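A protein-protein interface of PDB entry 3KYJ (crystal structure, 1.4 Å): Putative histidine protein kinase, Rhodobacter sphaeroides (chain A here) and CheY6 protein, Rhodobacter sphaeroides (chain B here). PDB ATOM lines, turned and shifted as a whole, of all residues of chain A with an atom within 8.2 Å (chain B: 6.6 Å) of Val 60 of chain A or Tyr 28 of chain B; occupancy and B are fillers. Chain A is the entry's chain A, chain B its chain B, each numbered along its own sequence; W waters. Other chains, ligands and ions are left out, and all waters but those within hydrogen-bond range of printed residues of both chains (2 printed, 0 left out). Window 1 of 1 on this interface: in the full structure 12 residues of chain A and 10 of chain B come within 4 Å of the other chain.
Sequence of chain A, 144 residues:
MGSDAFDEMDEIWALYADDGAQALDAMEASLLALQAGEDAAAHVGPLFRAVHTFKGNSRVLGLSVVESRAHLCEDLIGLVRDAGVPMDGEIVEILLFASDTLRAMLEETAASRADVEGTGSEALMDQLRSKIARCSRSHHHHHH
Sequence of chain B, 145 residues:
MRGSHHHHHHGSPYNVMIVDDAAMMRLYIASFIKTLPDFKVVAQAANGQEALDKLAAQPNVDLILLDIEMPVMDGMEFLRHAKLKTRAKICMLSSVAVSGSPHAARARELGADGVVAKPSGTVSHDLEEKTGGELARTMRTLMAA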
ATOM      1  N   MET A   9       3.729  -4.615   7.720  1.00  0.00           N
ATOM      2  CA  MET A   9       3.792  -5.761   6.812  1.00  0.00           C
ATOM      3  C   MET A   9       4.790  -5.557   5.677  1.00  0.00           C
ATOM      4  O   MET A   9       5.237  -6.529   5.062  1.00  0.00           O
ATOM      5  CB  MET A   9       2.409  -6.077   6.229  1.00  0.00           C
ATOM      6  CG  MET A   9       1.422  -6.686   7.239  1.00  0.00           C
ATOM      7  SD  MET A   9       2.040  -8.152   8.120  1.00  0.00           S
ATOM      8  CE  MET A   9       2.359  -7.490   9.756  1.00  0.00           C
ATOM      9  N   ILE A  12       8.050  -7.555   6.502  1.00  0.00           N
ATOM     10  CA  ILE A  12       8.063  -9.005   6.394  1.00  0.00           C
ATOM     11  C   ILE A  12       8.008  -9.446   4.935  1.00  0.00           C
ATOM     12  O   ILE A  12       8.645 -10.423   4.571  1.00  0.00           O
ATOM     13  CB  ILE A  12       6.971  -9.670   7.266  1.00  0.00           C
ATOM     14  CG1 ILE A  12       7.235 -11.177   7.363  1.00  0.00           C
ATOM     15  CG2 ILE A  12       5.575  -9.399   6.730  1.00  0.00           C
ATOM     16  CD1 ILE A  12       6.488 -11.867   8.497  1.00  0.00           C
ATOM     17  N   TRP A  13       7.298  -8.707   4.084  1.00  0.00           N
ATOM     18  CA  TRP A  13       7.293  -9.049   2.667  1.00  0.00           C
ATOM     19  C   TRP A  13       8.662  -8.797   2.015  1.00  0.00           C
ATOM     20  O   TRP A  13       9.090  -9.565   1.162  1.00  0.00           O
ATOM     21  CB  TRP A  13       6.144  -8.342   1.917  1.00  0.00           C
ATOM     22  CG  TRP A  13       4.854  -9.039   2.156  1.00  0.00           C
ATOM     23  CD1 TRP A  13       3.852  -8.660   2.999  1.00  0.00           C
ATOM     24  CD2 TRP A  13       4.454 -10.290   1.599  1.00  0.00           C
ATOM     25  NE1 TRP A  13       2.845  -9.588   2.980  1.00  0.00           N
ATOM     26  CE2 TRP A  13       3.201 -10.606   2.137  1.00  0.00           C
ATOM     27  CE3 TRP A  13       5.047 -11.186   0.700  1.00  0.00           C
ATOM     28  CZ2 TRP A  13       2.506 -11.764   1.784  1.00  0.00           C
ATOM     29  CZ3 TRP A  13       4.344 -12.328   0.341  1.00  0.00           C
ATOM     30  CH2 TRP A  13       3.088 -12.608   0.895  1.00  0.00           C
ATOM     31  N   LEU A  15      11.515  -9.052   3.601  1.00  0.00           N
ATOM     32  CA  LEU A  15      12.350 -10.134   4.096  1.00  0.00           C
ATOM     33  C   LEU A  15      12.028 -11.452   3.392  1.00  0.00           C
ATOM     34  O   LEU A  15      12.917 -12.236   3.096  1.00  0.00           O
ATOM     35  CB  LEU A  15      12.182 -10.261   5.603  1.00  0.00           C
ATOM     36  CG  LEU A  15      13.019 -11.347   6.244  1.00  0.00           C
ATOM     37  CD1 LEU A  15      14.500 -11.024   6.015  1.00  0.00           C
ATOM     38  CD2 LEU A  15      12.700 -11.421   7.739  1.00  0.00           C
ATOM     39  N   TYR A  16      10.759 -11.699   3.116  1.00  0.00           N
ATOM     40  CA  TYR A  16      10.388 -12.899   2.370  1.00  0.00           C
ATOM     41  C   TYR A  16      11.105 -12.947   1.025  1.00  0.00           C
ATOM     42  O   TYR A  16      11.638 -13.973   0.617  1.00  0.00           O
ATOM     43  CB  TYR A  16       8.874 -12.918   2.191  1.00  0.00           C
ATOM     44  CG  TYR A  16       8.336 -13.944   1.240  1.00  0.00           C
ATOM     45  CD1 TYR A  16       8.243 -15.290   1.599  1.00  0.00           C
ATOM     46  CD2 TYR A  16       7.854 -13.551  -0.012  1.00  0.00           C
ATOM     47  CE1 TYR A  16       7.711 -16.225   0.714  1.00  0.00           C
ATOM     48  CE2 TYR A  16       7.351 -14.472  -0.894  1.00  0.00           C
ATOM     49  CZ  TYR A  16       7.268 -15.790  -0.525  1.00  0.00           C
ATOM     50  OH  TYR A  16       6.721 -16.678  -1.420  1.00  0.00           O
ATOM     51  N   THR A  53      14.362 -23.943   4.523  1.00  0.00           N
ATOM     52  CA  THR A  53      14.207 -22.532   4.813  1.00  0.00           C
ATOM     53  C   THR A  53      13.127 -21.906   3.919  1.00  0.00           C
ATOM     54  O   THR A  53      12.237 -21.171   4.383  1.00  0.00           O
ATOM     55  CB  THR A  53      15.539 -21.811   4.590  1.00  0.00           C
ATOM     56  OG1 THR A  53      16.432 -22.204   5.630  1.00  0.00           O
ATOM     57  CG2 THR A  53      15.357 -20.287   4.607  1.00  0.00           C
ATOM     58  N   PHE A  54      13.198 -22.183   2.619  1.00  0.00           N
ATOM     59  CA  PHE A  54      12.221 -21.630   1.702  1.00  0.00           C
ATOM     60  C   PHE A  54      10.797 -22.079   2.072  1.00  0.00           C
ATOM     61  O   PHE A  54       9.867 -21.276   2.101  1.00  0.00           O
ATOM     62  CB  PHE A  54      12.590 -22.004   0.276  1.00  0.00           C
ATOM     63  CG  PHE A  54      11.785 -21.262  -0.745  1.00  0.00           C
ATOM     64  CD1 PHE A  54      12.213 -20.047  -1.229  1.00  0.00           C
ATOM     65  CD2 PHE A  54      10.573 -21.761  -1.173  1.00  0.00           C
ATOM     66  CE1 PHE A  54      11.461 -19.345  -2.152  1.00  0.00           C
ATOM     67  CE2 PHE A  54       9.802 -21.058  -2.084  1.00  0.00           C
ATOM     68  CZ  PHE A  54      10.239 -19.856  -2.574  1.00  0.00           C
ATOM     69  N   LYS A  55      10.653 -23.356   2.398  1.00  0.00           N
ATOM     70  CA  LYS A  55       9.391 -23.895   2.856  1.00  0.00           C
ATOM     71  C   LYS A  55       8.875 -23.191   4.117  1.00  0.00           C
ATOM     72  O   LYS A  55       7.714 -22.774   4.179  1.00  0.00           O
ATOM     73  CB  LYS A  55       9.536 -25.388   3.123  1.00  0.00           C
ATOM     74  CG  LYS A  55       8.239 -26.080   3.473  1.00  0.00           C
ATOM     75  CD  LYS A  55       8.404 -27.529   3.978  1.00  0.00           C
ATOM     76  CE  LYS A  55       8.862 -27.540   5.425  1.00  0.00           C
ATOM     77  NZ  LYS A  55       8.782 -28.903   6.026  1.00  0.00           N
ATOM     78  N   GLY A  56       9.713 -23.076   5.133  1.00  0.00           N
ATOM     79  CA  GLY A  56       9.305 -22.421   6.364  1.00  0.00           C
ATOM     80  C   GLY A  56       8.919 -20.964   6.177  1.00  0.00           C
ATOM     81  O   GLY A  56       7.995 -20.477   6.807  1.00  0.00           O
ATOM     82  N   ASN A  57       9.627 -20.276   5.289  1.00  0.00           N
ATOM     83  CA  ASN A  57       9.343 -18.873   5.003  1.00  0.00           C
ATOM     84  C   ASN A  57       7.936 -18.728   4.403  1.00  0.00           C
ATOM     85  O   ASN A  57       7.171 -17.847   4.761  1.00  0.00           O
ATOM     86  CB  ASN A  57      10.394 -18.304   4.030  1.00  0.00           C
ATOM     87  CG  ASN A  57      11.761 -18.068   4.667  1.00  0.00           C
ATOM     88  OD1 ASN A  57      11.993 -18.365   5.843  1.00  0.00           O
ATOM     89  ND2 ASN A  57      12.671 -17.535   3.877  1.00  0.00           N
ATOM     90  N   SER A  58       7.607 -19.618   3.471  1.00  0.00           N
ATOM     91  CA  SER A  58       6.306 -19.562   2.838  1.00  0.00           C
ATOM     92  C   SER A  58       5.212 -19.917   3.840  1.00  0.00           C
ATOM     93  O   SER A  58       4.119 -19.344   3.799  1.00  0.00           O
ATOM     94  CB  SER A  58       6.263 -20.482   1.616  1.00  0.00           C
ATOM     95  OG  SER A  58       6.295 -21.867   1.956  1.00  0.00           O
ATOM     96  N   ARG A  59       5.501 -20.841   4.751  1.00  0.00           N
ATOM     97  CA  ARG A  59       4.544 -21.201   5.778  1.00  0.00           C
ATOM     98  C   ARG A  59       4.235 -20.013   6.701  1.00  0.00           C
ATOM     99  O   ARG A  59       3.082 -19.825   7.071  1.00  0.00           O
ATOM    100  CB  ARG A  59       5.049 -22.409   6.563  1.00  0.00           C
ATOM    101  CG  ARG A  59       4.115 -22.859   7.692  1.00  0.00           C
ATOM    102  CD  ARG A  59       4.723 -24.024   8.480  1.00  0.00           C
ATOM    103  NE  ARG A  59       4.941 -25.178   7.614  1.00  0.00           N
ATOM    104  CZ  ARG A  59       5.677 -26.247   7.918  1.00  0.00           C
ATOM    105  NH1 ARG A  59       6.300 -26.334   9.091  1.00  0.00           N
ATOM    106  NH2 ARG A  59       5.801 -27.235   7.035  1.00  0.00           N
ATOM    107  N   VAL A  60       5.246 -19.219   7.073  1.00  0.00           N
ATOM    108  CA  VAL A  60       5.046 -18.048   7.938  1.00  0.00           C
ATOM    109  C   VAL A  60       3.953 -17.137   7.383  1.00  0.00           C
ATOM    110  O   VAL A  60       3.164 -16.576   8.140  1.00  0.00           O
ATOM    111  CB  VAL A  60       6.398 -17.244   8.119  1.00  0.00           C
ATOM    112  CG1 VAL A  60       6.159 -15.819   8.698  1.00  0.00           C
ATOM    113  CG2 VAL A  60       7.325 -17.988   9.027  1.00  0.00           C
ATOM    114  N   LEU A  61       3.968 -16.954   6.072  1.00  0.00           N
ATOM    115  CA  LEU A  61       3.052 -16.045   5.396  1.00  0.00           C
ATOM    116  C   LEU A  61       1.776 -16.735   4.905  1.00  0.00           C
ATOM    117  O   LEU A  61       0.970 -16.090   4.238  1.00  0.00           O
ATOM    118  CB  LEU A  61       3.764 -15.304   4.255  1.00  0.00           C
ATOM    119  CG  LEU A  61       4.796 -14.269   4.761  1.00  0.00           C
ATOM    120  CD1 LEU A  61       5.606 -13.618   3.663  1.00  0.00           C
ATOM    121  CD2 LEU A  61       4.051 -13.197   5.575  1.00  0.00           C
ATOM    122  N   GLY A  62       1.590 -18.012   5.241  1.00  0.00           N
ATOM    123  CA  GLY A  62       0.391 -18.750   4.896  1.00  0.00           C
ATOM    124  C   GLY A  62       0.262 -19.070   3.421  1.00  0.00           C
ATOM    125  O   GLY A  62      -0.853 -19.240   2.920  1.00  0.00           O
ATOM    126  N   LEU A  63       1.386 -19.182   2.719  1.00  0.00           N
ATOM    127  CA  LEU A  63       1.377 -19.392   1.268  1.00  0.00           C
ATOM    128  C   LEU A  63       1.403 -20.894   1.022  1.00  0.00           C
ATOM    129  O   LEU A  63       2.410 -21.454   0.615  1.00  0.00           O
ATOM    130  CB  LEU A  63       2.549 -18.659   0.611  1.00  0.00           C
ATOM    131  CG  LEU A  63       2.700 -17.192   1.009  1.00  0.00           C
ATOM    132  CD1 LEU A  63       3.945 -16.556   0.391  1.00  0.00           C
ATOM    133  CD2 LEU A  63       1.442 -16.416   0.629  1.00  0.00           C
ATOM    134  N   SER A  64       0.258 -21.531   1.244  1.00  0.00           N
ATOM    135  CA  SER A  64       0.175 -22.990   1.272  1.00  0.00           C
ATOM    136  C   SER A  64       0.485 -23.657  -0.080  1.00  0.00           C
ATOM    137  O   SER A  64       1.026 -24.764  -0.092  1.00  0.00           O
ATOM    138  CB  SER A  64      -1.207 -23.451   1.776  1.00  0.00           C
ATOM    139  OG  SER A  64      -1.467 -23.052   3.127  1.00  0.00           O
ATOM    140  N   GLU A  67       4.255 -23.440  -0.332  1.00  0.00           N
ATOM    141  CA  GLU A  67       4.743 -24.359   0.675  1.00  0.00           C
ATOM    142  C   GLU A  67       4.690 -25.798   0.177  1.00  0.00           C
ATOM    143  O   GLU A  67       5.626 -26.552   0.366  1.00  0.00           O
ATOM    144  CB  GLU A  67       3.940 -24.199   1.958  1.00  0.00           C
ATOM    145  CG  GLU A  67       4.432 -25.058   3.113  1.00  0.00           C
ATOM    146  CD  GLU A  67       3.563 -24.965   4.340  1.00  0.00           C
ATOM    147  OE1 GLU A  67       2.638 -24.141   4.375  1.00  0.00           O
ATOM    148  OE2 GLU A  67       3.789 -25.738   5.271  1.00  0.00           O
ATOM    149  N   ILE B  18      14.470 -13.878  21.354  1.00  0.00           N
ATOM    150  CA  ILE B  18      14.055 -14.847  20.327  1.00  0.00           C
ATOM    151  C   ILE B  18      15.309 -15.388  19.626  1.00  0.00           C
ATOM    152  O   ILE B  18      16.107 -14.606  19.116  1.00  0.00           O
ATOM    153  CB  ILE B  18      13.169 -14.205  19.254  1.00  0.00           C
ATOM    154  CG1 ILE B  18      11.947 -13.530  19.875  1.00  0.00           C
ATOM    155  CG2 ILE B  18      12.741 -15.235  18.230  1.00  0.00           C
ATOM    156  CD1 ILE B  18      11.251 -12.565  18.938  1.00  0.00           C
ATOM    157  N   ALA B  23      15.301 -15.846   9.917  1.00  0.00           N
ATOM    158  CA  ALA B  23      14.953 -14.447  10.064  1.00  0.00           C
ATOM    159  C   ALA B  23      13.452 -14.200   9.944  1.00  0.00           C
ATOM    160  O   ALA B  23      12.920 -13.358  10.628  1.00  0.00           O
ATOM    161  CB  ALA B  23      15.671 -13.642   9.029  1.00  0.00           C
ATOM    162  N   MET B  24      12.744 -14.932   9.093  1.00  0.00           N
ATOM    163  CA  MET B  24      11.297 -14.735   8.977  1.00  0.00           C
ATOM    164  C   MET B  24      10.562 -15.104  10.249  1.00  0.00           C
ATOM    165  O   MET B  24       9.594 -14.439  10.636  1.00  0.00           O
ATOM    166  CB  MET B  24      10.698 -15.570   7.830  1.00  0.00           C
ATOM    167  CG  MET B  24      11.006 -15.042   6.441  1.00  0.00           C
ATOM    168  SD  MET B  24      10.126 -13.557   6.013  1.00  0.00           S
ATOM    169  CE  MET B  24       8.534 -14.329   5.802  1.00  0.00           C
ATOM    170  N   MET B  25      11.010 -16.153  10.912  1.00  0.00           N
ATOM    171  CA  MET B  25      10.360 -16.558  12.144  1.00  0.00           C
ATOM    172  C   MET B  25      10.676 -15.551  13.269  1.00  0.00           C
ATOM    173  O   MET B  25       9.801 -15.209  14.056  1.00  0.00           O
ATOM    174  CB  MET B  25      10.780 -17.964  12.527  1.00  0.00           C
ATOM    175  CG  MET B  25      10.046 -18.512  13.769  1.00  0.00           C
ATOM    176  SD  MET B  25       8.245 -18.520  13.704  1.00  0.00           S
ATOM    177  CE  MET B  25       7.971 -19.586  12.324  1.00  0.00           C
ATOM    178  N   ARG B  26      11.902 -15.047  13.318  1.00  0.00           N
ATOM    179  CA  ARG B  26      12.231 -14.035  14.329  1.00  0.00           C
ATOM    180  C   ARG B  26      11.352 -12.795  14.151  1.00  0.00           C
ATOM    181  O   ARG B  26      10.818 -12.269  15.111  1.00  0.00           O
ATOM    182  CB  ARG B  26      13.713 -13.631  14.294  1.00  0.00           C
ATOM    183  CG  ARG B  26      14.673 -14.759  14.529  1.00  0.00           C
ATOM    184  CD  ARG B  26      16.096 -14.252  14.893  1.00  0.00           C
ATOM    185  NE  ARG B  26      16.690 -13.410  13.852  1.00  0.00           N
ATOM    186  CZ  ARG B  26      17.333 -13.854  12.773  1.00  0.00           C
ATOM    187  NH1 ARG B  26      17.474 -15.151  12.536  1.00  0.00           N
ATOM    188  NH2 ARG B  26      17.853 -12.983  11.908  1.00  0.00           N
ATOM    189  N   LEU B  27      11.201 -12.320  12.918  1.00  0.00           N
ATOM    190  CA  LEU B  27      10.398 -11.124  12.663  1.00  0.00           C
ATOM    191  C   LEU B  27       8.920 -11.386  12.958  1.00  0.00           C
ATOM    192  O   LEU B  27       8.246 -10.568  13.575  1.00  0.00           O
ATOM    193  CB  LEU B  27      10.566 -10.687  11.206  1.00  0.00           C
ATOM    194  CG  LEU B  27       9.732  -9.467  10.824  1.00  0.00           C
ATOM    195  CD1 LEU B  27       9.938  -8.265  11.738  1.00  0.00           C
ATOM    196  CD2 LEU B  27      10.061  -9.123   9.366  1.00  0.00           C
ATOM    197  N   TYR B  28       8.421 -12.540  12.547  1.00  0.00           N
ATOM    198  CA  TYR B  28       7.018 -12.874  12.773  1.00  0.00           C
ATOM    199  C   TYR B  28       6.677 -12.937  14.255  1.00  0.00           C
ATOM    200  O   TYR B  28       5.693 -12.339  14.719  1.00  0.00           O
ATOM    201  CB  TYR B  28       6.701 -14.209  12.096  1.00  0.00           C
ATOM    202  CG  TYR B  28       5.232 -14.583  12.129  1.00  0.00           C
ATOM    203  CD1 TYR B  28       4.347 -14.029  11.237  1.00  0.00           C
ATOM    204  CD2 TYR B  28       4.753 -15.503  13.031  1.00  0.00           C
ATOM    205  CE1 TYR B  28       3.003 -14.379  11.239  1.00  0.00           C
ATOM    206  CE2 TYR B  28       3.404 -15.853  13.058  1.00  0.00           C
ATOM    207  CZ  TYR B  28       2.543 -15.287  12.144  1.00  0.00           C
ATOM    208  OH  TYR B  28       1.197 -15.615  12.127  1.00  0.00           O
ATOM    209  N   ILE B  29       7.521 -13.623  15.020  1.00  0.00           N
ATOM    210  CA  ILE B  29       7.309 -13.721  16.448  1.00  0.00           C
ATOM    211  C   ILE B  29       7.481 -12.349  17.099  1.00  0.00           C
ATOM    212  O   ILE B  29       6.680 -11.977  17.966  1.00  0.00           O
ATOM    213  CB  ILE B  29       8.229 -14.771  17.093  1.00  0.00           C
ATOM    214  CG1 ILE B  29       7.792 -16.152  16.627  1.00  0.00           C
ATOM    215  CG2 ILE B  29       8.149 -14.693  18.636  1.00  0.00           C
ATOM    216  CD1 ILE B  29       8.653 -17.306  17.129  1.00  0.00           C
ATOM    217  N   ALA B  30       8.492 -11.584  16.692  1.00  0.00           N
ATOM    218  CA  ALA B  30       8.693 -10.258  17.274  1.00  0.00           C
ATOM    219  C   ALA B  30       7.477  -9.365  17.015  1.00  0.00           C
ATOM    220  O   ALA B  30       7.042  -8.621  17.910  1.00  0.00           O
ATOM    221  CB  ALA B  30       9.971  -9.599  16.742  1.00  0.00           C
ATOM    222  N   SER B  31       6.933  -9.426  15.802  1.00  0.00           N
ATOM    223  CA  SER B  31       5.783  -8.599  15.462  1.00  0.00           C
ATOM    224  C   SER B  31       4.584  -8.968  16.326  1.00  0.00           C
ATOM    225  O   SER B  31       3.821  -8.104  16.773  1.00  0.00           O
ATOM    226  CB  SER B  31       5.445  -8.735  13.983  1.00  0.00           C
ATOM    227  OG  SER B  31       6.462  -8.153  13.194  1.00  0.00           O
ATOM    228  N   PHE B  32       4.406 -10.260  16.551  1.00  0.00           N
ATOM    229  CA  PHE B  32       3.354 -10.711  17.416  1.00  0.00           C
ATOM    230  C   PHE B  32       3.530 -10.245  18.870  1.00  0.00           C
ATOM    231  O   PHE B  32       2.582  -9.778  19.506  1.00  0.00           O
ATOM    232  CB  PHE B  32       3.208 -12.202  17.366  1.00  0.00           C
ATOM    233  CG  PHE B  32       2.109 -12.701  18.252  1.00  0.00           C
ATOM    234  CD1 PHE B  32       0.782 -12.370  17.980  1.00  0.00           C
ATOM    235  CD2 PHE B  32       2.398 -13.474  19.355  1.00  0.00           C
ATOM    236  CE1 PHE B  32      -0.239 -12.836  18.806  1.00  0.00           C
ATOM    237  CE2 PHE B  32       1.387 -13.941  20.193  1.00  0.00           C
ATOM    238  CZ  PHE B  32       0.063 -13.607  19.918  1.00  0.00           C
ATOM    239  N   ILE B  33       4.742 -10.363  19.397  1.00  0.00           N
ATOM    240  CA  ILE B  33       4.989  -9.924  20.771  1.00  0.00           C
ATOM    241  C   ILE B  33       4.752  -8.440  20.950  1.00  0.00           C
ATOM    242  O   ILE B  33       4.316  -8.025  22.031  1.00  0.00           O
ATOM    243  CB  ILE B  33       6.405 -10.338  21.197  1.00  0.00           C
ATOM    244  CG1 ILE B  33       6.393 -11.869  21.368  1.00  0.00           C
ATOM    245  CG2 ILE B  33       6.825  -9.613  22.485  1.00  0.00           C
ATOM    246  CD1 ILE B  33       7.752 -12.513  21.656  1.00  0.00           C
ATOM    247  N   LYS B 118       5.634 -23.386  16.482  1.00  0.00           N
ATOM    248  CA  LYS B 118       5.824 -22.088  15.893  1.00  0.00           C
ATOM    249  C   LYS B 118       4.514 -21.641  15.283  1.00  0.00           C
ATOM    250  O   LYS B 118       3.816 -22.439  14.664  1.00  0.00           O
ATOM    251  CB  LYS B 118       6.906 -22.148  14.818  1.00  0.00           C
ATOM    252  CG  LYS B 118       8.286 -22.288  15.376  1.00  0.00           C
ATOM    253  CD  LYS B 118       9.311 -22.612  14.291  1.00  0.00           C
ATOM    254  CE  LYS B 118      10.583 -23.103  14.937  1.00  0.00           C
ATOM    255  NZ  LYS B 118      11.697 -23.234  13.949  1.00  0.00           N
ATOM    256  N   PRO B 119       4.182 -20.360  15.447  1.00  0.00           N
ATOM    257  CA  PRO B 119       2.969 -19.846  14.800  1.00  0.00           C
ATOM    258  C   PRO B 119       3.141 -19.673  13.290  1.00  0.00           C
ATOM    259  O   PRO B 119       4.252 -19.664  12.766  1.00  0.00           O
ATOM    260  CB  PRO B 119       2.782 -18.479  15.471  1.00  0.00           C
ATOM    261  CG  PRO B 119       4.170 -18.035  15.810  1.00  0.00           C
ATOM    262  CD  PRO B 119       4.899 -19.311  16.201  1.00  0.00           C
ATOM    263  N   SER B 120       2.028 -19.524  12.589  1.00  0.00           N
ATOM    264  CA  SER B 120       2.076 -19.239  11.157  1.00  0.00           C
ATOM    265  C   SER B 120       0.844 -18.479  10.681  1.00  0.00           C
ATOM    266  O   SER B 120      -0.182 -18.486  11.343  1.00  0.00           O
ATOM    267  CB  SER B 120       2.196 -20.539  10.373  1.00  0.00           C
ATOM    268  OG  SER B 120       1.016 -21.303  10.497  1.00  0.00           O
ATOM    269  N   GLY B 121       0.949 -17.843   9.517  1.00  0.00           N
ATOM    270  CA  GLY B 121      -0.198 -17.190   8.889  1.00  0.00           C
ATOM    271  C   GLY B 121      -1.032 -18.171   8.080  1.00  0.00           C
ATOM    272  O   GLY B 121      -1.894 -17.765   7.300  1.00  0.00           O
ATOM    273  N   THR B 122      -0.783 -19.462   8.291  1.00  0.00           N
ATOM    274  CA  THR B 122      -1.408 -20.545   7.523  1.00  0.00           C
ATOM    275  C   THR B 122      -2.867 -20.798   7.911  1.00  0.00           C
ATOM    276  O   THR B 122      -3.357 -20.267   8.911  1.00  0.00           O
ATOM    277  CB  THR B 122      -0.605 -21.871   7.721  1.00  0.00           C
ATOM    278  OG1 THR B 122       0.729 -21.708   7.229  1.00  0.00           O
ATOM    279  CG2 THR B 122      -1.252 -23.053   7.002  1.00  0.00           C
ATOM    280  N   THR B 131      -3.837 -16.807  15.302  1.00  0.00           N
ATOM    281  CA  THR B 131      -2.376 -16.684  15.072  1.00  0.00           C
ATOM    282  C   THR B 131      -1.221 -16.942  16.045  1.00  0.00           C
ATOM    283  O   THR B 131      -0.145 -17.423  15.689  1.00  0.00           O
ATOM    284  CB  THR B 131      -1.995 -15.175  14.928  1.00  0.00           C
ATOM    285  OG1 THR B 131      -2.459 -14.450  16.077  1.00  0.00           O
ATOM    286  CG2 THR B 131      -2.617 -14.564  13.679  1.00  0.00           C
ATOM    287  N   GLY B 132      -1.334 -16.653  17.218  1.00  0.00           N
ATOM    288  CA  GLY B 132      -0.299 -16.796  18.205  1.00  0.00           C
ATOM    289  C   GLY B 132      -1.027 -16.983  19.518  1.00  0.00           C
ATOM    290  O   GLY B 132      -0.476 -16.834  20.575  1.00  0.00           O
HETATM  291  O   HOH W   1      13.825 -16.959   7.280  1.00  0.00           O
HETATM  292  O   HOH W   2       0.948 -22.353   4.558  1.00  0.00           O
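CD2 of Leu 15 of chain A touches O of Ala 23 of chain B, at 3.5 Å. Met 24 of chain B touches Leu 15 of chain A. Met 24 of chain B touches Asn 57 of chain A. Ser 120 of chain B touches Arg 59 of chain A. Arg 59 of chain A touches Gly 121 of chain B. Val 60 of chain A touches Met 25 of chain B. CG1 of Val 60 of chain A touches CD1 of Tyr 28 of chain B (3.6 Å). Met 24 of chain B touches Leu 61 of chain A. O of Gly 121 of chain B touches CA of Gly 62 of chain A (3.5 Å). Gly 62 of chain A touches Thr 122 of chain B.
Water W2 lies within hydrogen-bond range of OE1 of Glu 67 of chain A (2.5 Å), OG1 of Thr 122 of chain B (2.8 Å) and OG of Ser 64 of chain A (2.9 Å). Water W1 lies within hydrogen-bond range of the side-chain amide oxygen (OD1) of Asn 57 of chain A (2.7 Å), the backbone NH (N) of Met 24 of chain B (2.9 Å) and the backbone NH (N) of Ala 23 of chain B (3.2 Å).
Of the 19 printed residues of chain B, 8 touch a printed residue of chain A. Hydrophobic or aromatic side chains of chain B within 4 Å of the printed part of chain A: Ala 23, Met 24, Met 25, Leu 27 and Tyr 28. Hydrophobic or aromatic side chains of chain A within 4 Å of the printed part of chain B: Ile 12, Leu 15, Tyr 16, Val 60 and Leu 61.
N of Gly 121 of chain B sits at hydrogen-bond distance from OH of Tyr 28 of chain B (3.4 Å). The side-chain hydroxyl (OH) of Tyr 28 of chain B sits close to the backbone carbonyl oxygen (O) of Ser 120 of chain B (3.3 Å). The guanidinium group (NE) of Arg 59 of chain A lies within salt-bridge range of the side-chain carboxylate (OE2) of Glu 67 of chain A, at 2.7 Å. The side-chain hydroxyl (OG) of Ser 31 of chain B lies within hydrogen-bond range of the backbone carbonyl oxygen (O) of Leu 27 of chain B (3.0 Å). The backbone carbonyl oxygen (O) of Thr 53 of chain A lies close to the side-chain amide oxygen (OD1) of Asn 57 of chain A. The side-chain hydroxyl (OG) of Ser 120 of chain B lies close to the side-chain hydroxyl (OG1) of Thr 122 of chain B, 3.3 Å away.
Val 60 of chain A touches four residues of chain B. Of chain A, only Val 60 comes within 4 Å of Tyr 28 of chain B. Of the printed residues of chain A, Met 25 of chain B touches Val 60 (3.7 Å). Of the printed residues of chain A, Ser 120 of chain B touches Arg 59 (3.5 Å) and Val 60 (3.9 Å). Printed residues of chain B within 4 Å of Ile 12 of chain A: Met 24 and Leu 27. Leu 63 of chain A touches none of the printed residues of chain B. The nearest printed residue of chain B that does not touch Val 60 of chain A is Met 24 of chain B (4.03 Å). The nearest residue of chain A that does not touch Tyr 28 of chain B is Ile 12 of chain A (4.1 Å).
O of Arg 59 of chain A lies within hydrogen-bond range of OG1 of Thr 122 of chain B, 3.0 Å away. O of Val 60 of chain A is in hydrogen-bond range of N of Gly 121 of chain B (2.9 Å). The backbone NH (N) of Tyr 16 of chain A is in hydrogen-bond range of the side-chain sulfur (SD) of Met 24 of chain B, 3.5 Å away. SD of Met 24 of chain B sits close to O of Ile 12 of chain A, 3.8 Å away.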
